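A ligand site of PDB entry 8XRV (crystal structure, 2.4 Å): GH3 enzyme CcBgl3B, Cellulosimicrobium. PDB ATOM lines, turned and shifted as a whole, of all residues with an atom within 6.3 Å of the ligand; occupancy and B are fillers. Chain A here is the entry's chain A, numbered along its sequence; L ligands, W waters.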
ATOM      1  N   LEU A  58     -19.456  -9.027 -13.981  1.00  0.00           N
ATOM      2  CA  LEU A  58     -20.191  -7.871 -14.475  1.00  0.00           C
ATOM      3  C   LEU A  58     -19.259  -7.024 -15.344  1.00  0.00           C
ATOM      4  O   LEU A  58     -18.036  -7.180 -15.333  1.00  0.00           O
ATOM      5  CB  LEU A  58     -20.790  -7.038 -13.345  1.00  0.00           C
ATOM      6  CG  LEU A  58     -19.899  -6.174 -12.448  1.00  0.00           C
ATOM      7  CD1 LEU A  58     -20.793  -5.176 -11.724  1.00  0.00           C
ATOM      8  CD2 LEU A  58     -19.191  -7.023 -11.436  1.00  0.00           C
ATOM      9  N   HIS A  59     -19.871  -6.119 -16.117  1.00  0.00           N
ATOM     10  CA  HIS A  59     -19.150  -5.283 -17.073  1.00  0.00           C
ATOM     11  C   HIS A  59     -18.339  -6.142 -18.037  1.00  0.00           C
ATOM     12  O   HIS A  59     -17.152  -5.909 -18.281  1.00  0.00           O
ATOM     13  CB  HIS A  59     -18.281  -4.245 -16.355  1.00  0.00           C
ATOM     14  CG  HIS A  59     -19.062  -3.196 -15.623  1.00  0.00           C
ATOM     15  ND1 HIS A  59     -20.387  -2.932 -15.893  1.00  0.00           N
ATOM     16  CD2 HIS A  59     -18.708  -2.354 -14.626  1.00  0.00           C
ATOM     17  CE1 HIS A  59     -20.815  -1.975 -15.092  1.00  0.00           C
ATOM     18  NE2 HIS A  59     -19.811  -1.607 -14.311  1.00  0.00           N
ATOM     19  N   GLU A  85     -25.243  -7.335 -15.652  1.00  0.00           N
ATOM     20  CA  GLU A  85     -24.908  -6.077 -16.299  1.00  0.00           C
ATOM     21  C   GLU A  85     -25.849  -4.993 -15.796  1.00  0.00           C
ATOM     22  O   GLU A  85     -26.952  -5.277 -15.337  1.00  0.00           O
ATOM     23  CB  GLU A  85     -24.981  -6.202 -17.831  1.00  0.00           C
ATOM     24  CG  GLU A  85     -24.342  -5.031 -18.584  1.00  0.00           C
ATOM     25  CD  GLU A  85     -22.904  -4.739 -18.132  1.00  0.00           C
ATOM     26  OE1 GLU A  85     -22.728  -4.026 -17.112  1.00  0.00           O
ATOM     27  OE2 GLU A  85     -21.951  -5.227 -18.787  1.00  0.00           O
ATOM     28  N   ASP A  86     -25.384  -3.740 -15.899  1.00  0.00           N
ATOM     29  CA  ASP A  86     -26.256  -2.579 -15.724  1.00  0.00           C
ATOM     30  C   ASP A  86     -26.965  -2.314 -17.048  1.00  0.00           C
ATOM     31  O   ASP A  86     -26.370  -1.817 -18.005  1.00  0.00           O
ATOM     32  CB  ASP A  86     -25.467  -1.360 -15.286  1.00  0.00           C
ATOM     33  CG  ASP A  86     -24.811  -1.546 -13.926  1.00  0.00           C
ATOM     34  OD1 ASP A  86     -25.544  -1.444 -12.911  1.00  0.00           O
ATOM     35  OD2 ASP A  86     -23.573  -1.772 -13.870  1.00  0.00           O
ATOM     36  N   ILE A  88     -29.999  -0.219 -17.663  1.00  0.00           N
ATOM     37  CA  ILE A  88     -30.722   0.640 -16.730  1.00  0.00           C
ATOM     38  C   ILE A  88     -31.916   1.330 -17.384  1.00  0.00           C
ATOM     39  O   ILE A  88     -32.911   1.639 -16.709  1.00  0.00           O
ATOM     40  CB  ILE A  88     -29.723   1.659 -16.145  1.00  0.00           C
ATOM     41  CG1 ILE A  88     -28.559   0.881 -15.490  1.00  0.00           C
ATOM     42  CG2 ILE A  88     -30.404   2.594 -15.186  1.00  0.00           C
ATOM     43  CD1 ILE A  88     -29.037  -0.252 -14.576  1.00  0.00           C
ATOM     44  N   PHE A 135     -28.950  -5.111 -13.232  1.00  0.00           N
ATOM     45  CA  PHE A 135     -28.990  -4.408 -11.949  1.00  0.00           C
ATOM     46  C   PHE A 135     -29.995  -3.256 -12.063  1.00  0.00           C
ATOM     47  O   PHE A 135     -29.648  -2.075 -12.143  1.00  0.00           O
ATOM     48  CB  PHE A 135     -27.604  -3.921 -11.576  1.00  0.00           C
ATOM     49  CG  PHE A 135     -26.635  -5.027 -11.317  1.00  0.00           C
ATOM     50  CD1 PHE A 135     -26.979  -6.093 -10.481  1.00  0.00           C
ATOM     51  CD2 PHE A 135     -25.369  -5.011 -11.900  1.00  0.00           C
ATOM     52  CE1 PHE A 135     -26.080  -7.101 -10.211  1.00  0.00           C
ATOM     53  CE2 PHE A 135     -24.459  -6.015 -11.622  1.00  0.00           C
ATOM     54  CZ  PHE A 135     -24.821  -7.068 -10.781  1.00  0.00           C
ATOM     55  N   VAL A 138     -34.242   0.721 -10.187  1.00  0.00           N
ATOM     56  CA  VAL A 138     -33.874   1.516  -9.021  1.00  0.00           C
ATOM     57  C   VAL A 138     -35.157   1.885  -8.298  1.00  0.00           C
ATOM     58  O   VAL A 138     -36.106   2.380  -8.906  1.00  0.00           O
ATOM     59  CB  VAL A 138     -33.088   2.766  -9.433  1.00  0.00           C
ATOM     60  CG1 VAL A 138     -32.933   3.726  -8.240  1.00  0.00           C
ATOM     61  CG2 VAL A 138     -31.739   2.417  -9.995  1.00  0.00           C
ATOM     62  N   ARG A 149     -27.857  11.081  -8.376  1.00  0.00           N
ATOM     63  CA  ARG A 149     -28.450   9.920  -9.029  1.00  0.00           C
ATOM     64  C   ARG A 149     -29.970  10.037  -9.171  1.00  0.00           C
ATOM     65  O   ARG A 149     -30.637   9.034  -9.460  1.00  0.00           O
ATOM     66  CB  ARG A 149     -28.047   8.646  -8.293  1.00  0.00           C
ATOM     67  CG  ARG A 149     -26.515   8.461  -8.240  1.00  0.00           C
ATOM     68  CD  ARG A 149     -26.081   7.113  -7.700  1.00  0.00           C
ATOM     69  NE  ARG A 149     -26.267   6.023  -8.667  1.00  0.00           N
ATOM     70  CZ  ARG A 149     -25.823   4.782  -8.482  1.00  0.00           C
ATOM     71  NH1 ARG A 149     -26.061   3.851  -9.398  1.00  0.00           N
ATOM     72  NH2 ARG A 149     -25.148   4.460  -7.391  1.00  0.00           N
ATOM     73  N   GLU A 152     -31.809   8.347 -11.957  1.00  0.00           N
ATOM     74  CA  GLU A 152     -32.040   6.909 -11.898  1.00  0.00           C
ATOM     75  C   GLU A 152     -33.338   6.544 -11.164  1.00  0.00           C
ATOM     76  O   GLU A 152     -33.722   5.372 -11.188  1.00  0.00           O
ATOM     77  CB  GLU A 152     -30.857   6.222 -11.232  1.00  0.00           C
ATOM     78  CG  GLU A 152     -29.595   6.275 -12.089  1.00  0.00           C
ATOM     79  CD  GLU A 152     -28.371   5.752 -11.370  1.00  0.00           C
ATOM     80  OE1 GLU A 152     -28.385   4.550 -10.977  1.00  0.00           O
ATOM     81  OE2 GLU A 152     -27.381   6.518 -11.200  1.00  0.00           O
ATOM     82  N   LYS A 188     -32.772  -2.388  -6.392  1.00  0.00           N
ATOM     83  CA  LYS A 188     -31.463  -1.778  -6.282  1.00  0.00           C
ATOM     84  C   LYS A 188     -31.473  -0.615  -5.307  1.00  0.00           C
ATOM     85  O   LYS A 188     -32.329   0.279  -5.398  1.00  0.00           O
ATOM     86  CB  LYS A 188     -30.966  -1.307  -7.650  1.00  0.00           C
ATOM     87  CG  LYS A 188     -29.560  -0.955  -7.670  1.00  0.00           C
ATOM     88  CD  LYS A 188     -29.008  -1.185  -9.051  1.00  0.00           C
ATOM     89  CE  LYS A 188     -29.145   0.027  -9.893  1.00  0.00           C
ATOM     90  NZ  LYS A 188     -28.072  -0.009 -10.908  1.00  0.00           N
ATOM     91  N   HIS A 189     -30.513  -0.674  -4.377  1.00  0.00           N
ATOM     92  CA  HIS A 189     -30.053   0.301  -3.396  1.00  0.00           C
ATOM     93  C   HIS A 189     -30.942   0.238  -2.161  1.00  0.00           C
ATOM     94  O   HIS A 189     -31.290   1.256  -1.560  1.00  0.00           O
ATOM     95  CB  HIS A 189     -29.951   1.678  -4.015  1.00  0.00           C
ATOM     96  CG  HIS A 189     -29.045   1.729  -5.193  1.00  0.00           C
ATOM     97  ND1 HIS A 189     -29.313   2.508  -6.297  1.00  0.00           N
ATOM     98  CD2 HIS A 189     -27.893   1.072  -5.462  1.00  0.00           C
ATOM     99  CE1 HIS A 189     -28.361   2.335  -7.201  1.00  0.00           C
ATOM    100  NE2 HIS A 189     -27.486   1.472  -6.721  1.00  0.00           N
ATOM    101  N   TYR A 193     -30.575   4.904   0.314  1.00  0.00           N
ATOM    102  CA  TYR A 193     -29.364   5.430  -0.299  1.00  0.00           C
ATOM    103  C   TYR A 193     -29.537   6.849  -0.863  1.00  0.00           C
ATOM    104  O   TYR A 193     -28.578   7.616  -0.911  1.00  0.00           O
ATOM    105  CB  TYR A 193     -28.914   4.416  -1.355  1.00  0.00           C
ATOM    106  CG  TYR A 193     -27.759   4.797  -2.230  1.00  0.00           C
ATOM    107  CD1 TYR A 193     -26.635   5.425  -1.728  1.00  0.00           C
ATOM    108  CD2 TYR A 193     -27.779   4.482  -3.590  1.00  0.00           C
ATOM    109  CE1 TYR A 193     -25.581   5.773  -2.552  1.00  0.00           C
ATOM    110  CE2 TYR A 193     -26.729   4.816  -4.413  1.00  0.00           C
ATOM    111  CZ  TYR A 193     -25.628   5.465  -3.905  1.00  0.00           C
ATOM    112  OH  TYR A 193     -24.582   5.801  -4.748  1.00  0.00           O
ATOM    113  N   MET A 232     -30.155  -5.633  -4.220  1.00  0.00           N
ATOM    114  CA  MET A 232     -28.830  -5.063  -4.034  1.00  0.00           C
ATOM    115  C   MET A 232     -28.772  -4.232  -2.765  1.00  0.00           C
ATOM    116  O   MET A 232     -29.613  -3.349  -2.563  1.00  0.00           O
ATOM    117  CB  MET A 232     -28.413  -4.206  -5.217  1.00  0.00           C
ATOM    118  CG  MET A 232     -26.936  -3.946  -5.217  1.00  0.00           C
ATOM    119  SD  MET A 232     -26.418  -2.743  -6.444  1.00  0.00           S
ATOM    120  CE  MET A 232     -26.177  -3.834  -7.847  1.00  0.00           C
ATOM    121  N   TYR A 235     -24.657   1.113  -0.533  1.00  0.00           N
ATOM    122  CA  TYR A 235     -23.371   1.589  -0.036  1.00  0.00           C
ATOM    123  C   TYR A 235     -23.442   2.118   1.399  1.00  0.00           C
ATOM    124  O   TYR A 235     -22.492   1.966   2.171  1.00  0.00           O
ATOM    125  CB  TYR A 235     -22.882   2.764  -0.887  1.00  0.00           C
ATOM    126  CG  TYR A 235     -22.404   2.517  -2.274  1.00  0.00           C
ATOM    127  CD1 TYR A 235     -21.457   1.534  -2.547  1.00  0.00           C
ATOM    128  CD2 TYR A 235     -22.875   3.297  -3.322  1.00  0.00           C
ATOM    129  CE1 TYR A 235     -20.984   1.346  -3.836  1.00  0.00           C
ATOM    130  CE2 TYR A 235     -22.421   3.122  -4.606  1.00  0.00           C
ATOM    131  CZ  TYR A 235     -21.467   2.137  -4.850  1.00  0.00           C
ATOM    132  OH  TYR A 235     -21.022   1.979  -6.131  1.00  0.00           O
ATOM    133  N   ASP A 267     -23.480  -3.807  -3.300  1.00  0.00           N
ATOM    134  CA  ASP A 267     -23.044  -2.816  -4.264  1.00  0.00           C
ATOM    135  C   ASP A 267     -21.517  -2.876  -4.398  1.00  0.00           C
ATOM    136  O   ASP A 267     -20.833  -3.653  -3.716  1.00  0.00           O
ATOM    137  CB  ASP A 267     -23.560  -1.441  -3.840  1.00  0.00           C
ATOM    138  CG  ASP A 267     -23.928  -0.563  -5.029  1.00  0.00           C
ATOM    139  OD1 ASP A 267     -23.276  -0.687  -6.108  1.00  0.00           O
ATOM    140  OD2 ASP A 267     -24.841   0.287  -4.875  1.00  0.00           O
ATOM    141  N   TRP A 268     -20.992  -2.047  -5.289  1.00  0.00           N
ATOM    142  CA  TRP A 268     -19.603  -2.085  -5.708  1.00  0.00           C
ATOM    143  C   TRP A 268     -18.606  -1.907  -4.568  1.00  0.00           C
ATOM    144  O   TRP A 268     -18.442  -0.788  -4.066  1.00  0.00           O
ATOM    145  CB  TRP A 268     -19.379  -1.010  -6.773  1.00  0.00           C
ATOM    146  CG  TRP A 268     -18.075  -1.114  -7.475  1.00  0.00           C
ATOM    147  CD1 TRP A 268     -16.843  -0.747  -6.993  1.00  0.00           C
ATOM    148  CD2 TRP A 268     -17.847  -1.632  -8.800  1.00  0.00           C
ATOM    149  NE1 TRP A 268     -15.872  -1.020  -7.927  1.00  0.00           N
ATOM    150  CE2 TRP A 268     -16.459  -1.554  -9.038  1.00  0.00           C
ATOM    151  CE3 TRP A 268     -18.687  -2.144  -9.801  1.00  0.00           C
ATOM    152  CZ2 TRP A 268     -15.879  -1.973 -10.252  1.00  0.00           C
ATOM    153  CZ3 TRP A 268     -18.108  -2.578 -11.006  1.00  0.00           C
ATOM    154  CH2 TRP A 268     -16.710  -2.488 -11.214  1.00  0.00           C
ATOM    155  N   MET A 300     -19.890  -8.119  -4.463  1.00  0.00           N
ATOM    156  CA  MET A 300     -19.520  -7.505  -5.732  1.00  0.00           C
ATOM    157  C   MET A 300     -18.176  -6.809  -5.604  1.00  0.00           C
ATOM    158  O   MET A 300     -17.959  -6.048  -4.653  1.00  0.00           O
ATOM    159  CB  MET A 300     -20.597  -6.517  -6.189  1.00  0.00           C
ATOM    160  CG  MET A 300     -20.386  -5.950  -7.569  1.00  0.00           C
ATOM    161  SD  MET A 300     -21.366  -4.439  -7.843  1.00  0.00           S
ATOM    162  CE  MET A 300     -23.000  -5.111  -8.047  1.00  0.00           C
ATOM    163  N   TRP A 426     -25.430   6.069 -17.450  1.00  0.00           N
ATOM    164  CA  TRP A 426     -25.731   4.643 -17.600  1.00  0.00           C
ATOM    165  C   TRP A 426     -26.183   4.315 -19.027  1.00  0.00           C
ATOM    166  O   TRP A 426     -27.192   3.642 -19.250  1.00  0.00           O
ATOM    167  CB  TRP A 426     -26.781   4.191 -16.589  1.00  0.00           C
ATOM    168  CG  TRP A 426     -26.285   4.295 -15.205  1.00  0.00           C
ATOM    169  CD1 TRP A 426     -26.633   5.217 -14.281  1.00  0.00           C
ATOM    170  CD2 TRP A 426     -25.291   3.452 -14.597  1.00  0.00           C
ATOM    171  NE1 TRP A 426     -25.940   5.007 -13.115  1.00  0.00           N
ATOM    172  CE2 TRP A 426     -25.103   3.928 -13.276  1.00  0.00           C
ATOM    173  CE3 TRP A 426     -24.532   2.357 -15.030  1.00  0.00           C
ATOM    174  CZ2 TRP A 426     -24.208   3.337 -12.385  1.00  0.00           C
ATOM    175  CZ3 TRP A 426     -23.647   1.761 -14.146  1.00  0.00           C
ATOM    176  CH2 TRP A 426     -23.490   2.245 -12.838  1.00  0.00           C
ATOM    177  N   GLN A 432     -18.939   3.692 -17.438  1.00  0.00           N
ATOM    178  CA  GLN A 432     -18.850   2.485 -16.647  1.00  0.00           C
ATOM    179  C   GLN A 432     -18.428   1.258 -17.463  1.00  0.00           C
ATOM    180  O   GLN A 432     -18.036   0.250 -16.872  1.00  0.00           O
ATOM    181  CB  GLN A 432     -20.192   2.240 -15.947  1.00  0.00           C
ATOM    182  CG  GLN A 432     -20.589   3.402 -15.018  1.00  0.00           C
ATOM    183  CD  GLN A 432     -21.542   4.460 -15.653  1.00  0.00           C
ATOM    184  OE1 GLN A 432     -21.556   4.670 -16.870  1.00  0.00           O
ATOM    185  NE2 GLN A 432     -22.338   5.104 -14.798  1.00  0.00           N
ATOM    186  N   GLU A 528     -22.809   9.013  -9.857  1.00  0.00           N
ATOM    187  CA  GLU A 528     -22.038   8.593  -8.701  1.00  0.00           C
ATOM    188  C   GLU A 528     -20.890   9.559  -8.431  1.00  0.00           C
ATOM    189  O   GLU A 528     -20.174   9.966  -9.349  1.00  0.00           O
ATOM    190  CB  GLU A 528     -21.488   7.187  -8.920  1.00  0.00           C
ATOM    191  CG  GLU A 528     -22.486   6.079  -8.667  1.00  0.00           C
ATOM    192  CD  GLU A 528     -21.845   4.686  -8.741  1.00  0.00           C
ATOM    193  OE1 GLU A 528     -21.180   4.286  -7.765  1.00  0.00           O
ATOM    194  OE2 GLU A 528     -22.046   3.994  -9.764  1.00  0.00           O
HETATM  195  C1  LIG L   1     -23.662   1.410  -8.618  1.00  0.00           C
HETATM  196  C2  LIG L   1     -24.767   0.462  -8.917  1.00  0.00           C
HETATM  197  C3  LIG L   1     -24.414  -0.483 -10.008  1.00  0.00           C
HETATM  198  C4  LIG L   1     -23.258  -1.390  -9.626  1.00  0.00           C
HETATM  199  C5  LIG L   1     -22.688  -2.114 -10.866  1.00  0.00           C
HETATM  200  C6  LIG L   1     -22.240   0.749  -8.671  1.00  0.00           C
HETATM  201  O1  LIG L   1     -21.364   1.318  -9.595  1.00  0.00           O
HETATM  202  O2  LIG L   1     -23.945   1.979  -7.297  1.00  0.00           O
HETATM  203  O3  LIG L   1     -25.933   1.166  -9.248  1.00  0.00           O
HETATM  204  O4  LIG L   1     -25.513  -1.308 -10.261  1.00  0.00           O
HETATM  205  O5  LIG L   1     -22.207  -0.713  -8.796  1.00  0.00           O
HETATM  206  O6  LIG L   1     -22.045  -1.213 -11.718  1.00  0.00           O
HETATM  207  O   HOH W   1     -20.215   0.395 -12.293  1.00  0.00           O
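OD1 of Asp 86 is in hydrogen-bond range of O4 of the ligand (2.7 Å). O3 of the ligand lies within hydrogen-bond range of NH1 of Arg 149, 2.7 Å away. The side-chain carboxylate (OE2) of Glu 528 lies within hydrogen-bond range of an oxygen (O1) of the ligand. An oxygen (O2) of the ligand sits at hydrogen-bond distance from the side-chain carboxylate of Asp 267 (3.0 Å). NZ of Lys 188 sits at hydrogen-bond distance from O4 of the ligand, at 2.9 Å. A ring nitrogen (NE2) of His 189 is in hydrogen-bond range of an oxygen (O3) of the ligand. OH of Tyr 235 sits close to O2 of the ligand (3.1 Å). A ring nitrogen (NE2) of His 59 sits at hydrogen-bond distance from an oxygen (O6) of the ligand (3.4 Å).
CD1 of Leu 58 touches C5 of the ligand, 3.7 Å away. CB of Phe 135 touches O4 of the ligand (3.6 Å). CE of Met 232 touches O4 of the ligand, 3.6 Å away. Trp 268 touches the ligand (CB to O5, 3.5 Å). Met 300 touches the ligand. Trp 426 touches the ligand. Hydrophobic or aromatic side chains that line the ligand: Leu 58, His 59, Phe 135, His 189, Met 232, Tyr 235, Trp 268, Met 300 and Trp 426. Of the 20 residues printed, 14 come within 4 Å of the ligand.
Water W1 lies within hydrogen-bond range of O6 of the ligand (2.5 Å) and NE2 of His 59 (2.9 Å).
The side-chain carboxylate of Glu 528 lies within salt-bridge range of the guanidinium group of Arg 149 (3.9 Å). OH of Tyr 193 sits at hydrogen-bond distance from NH2 of Arg 149, 3.0 Å away. NE2 of His 189 lies close to OD2 of Asp 267 (3.4 Å). The side-chain carboxylate (OD1) of Asp 267 sits at hydrogen-bond distance from the side-chain hydroxyl (OH) of Tyr 235. O of Phe 135 is in hydrogen-bond range of NZ of Lys 188 (2.9 Å). The backbone NH (N) of His 189 lies within hydrogen-bond range of the backbone carbonyl oxygen (O) of Met 232 (3.4 Å). A ring nitrogen (ND1) of His 59 sits at hydrogen-bond distance from the side-chain carboxylate (OE1) of Glu 85, 2.9 Å away. The backbone carbonyl oxygen (O) of Glu 85 lies within hydrogen-bond range of the backbone NH (N) of Phe 135 (2.9 Å).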
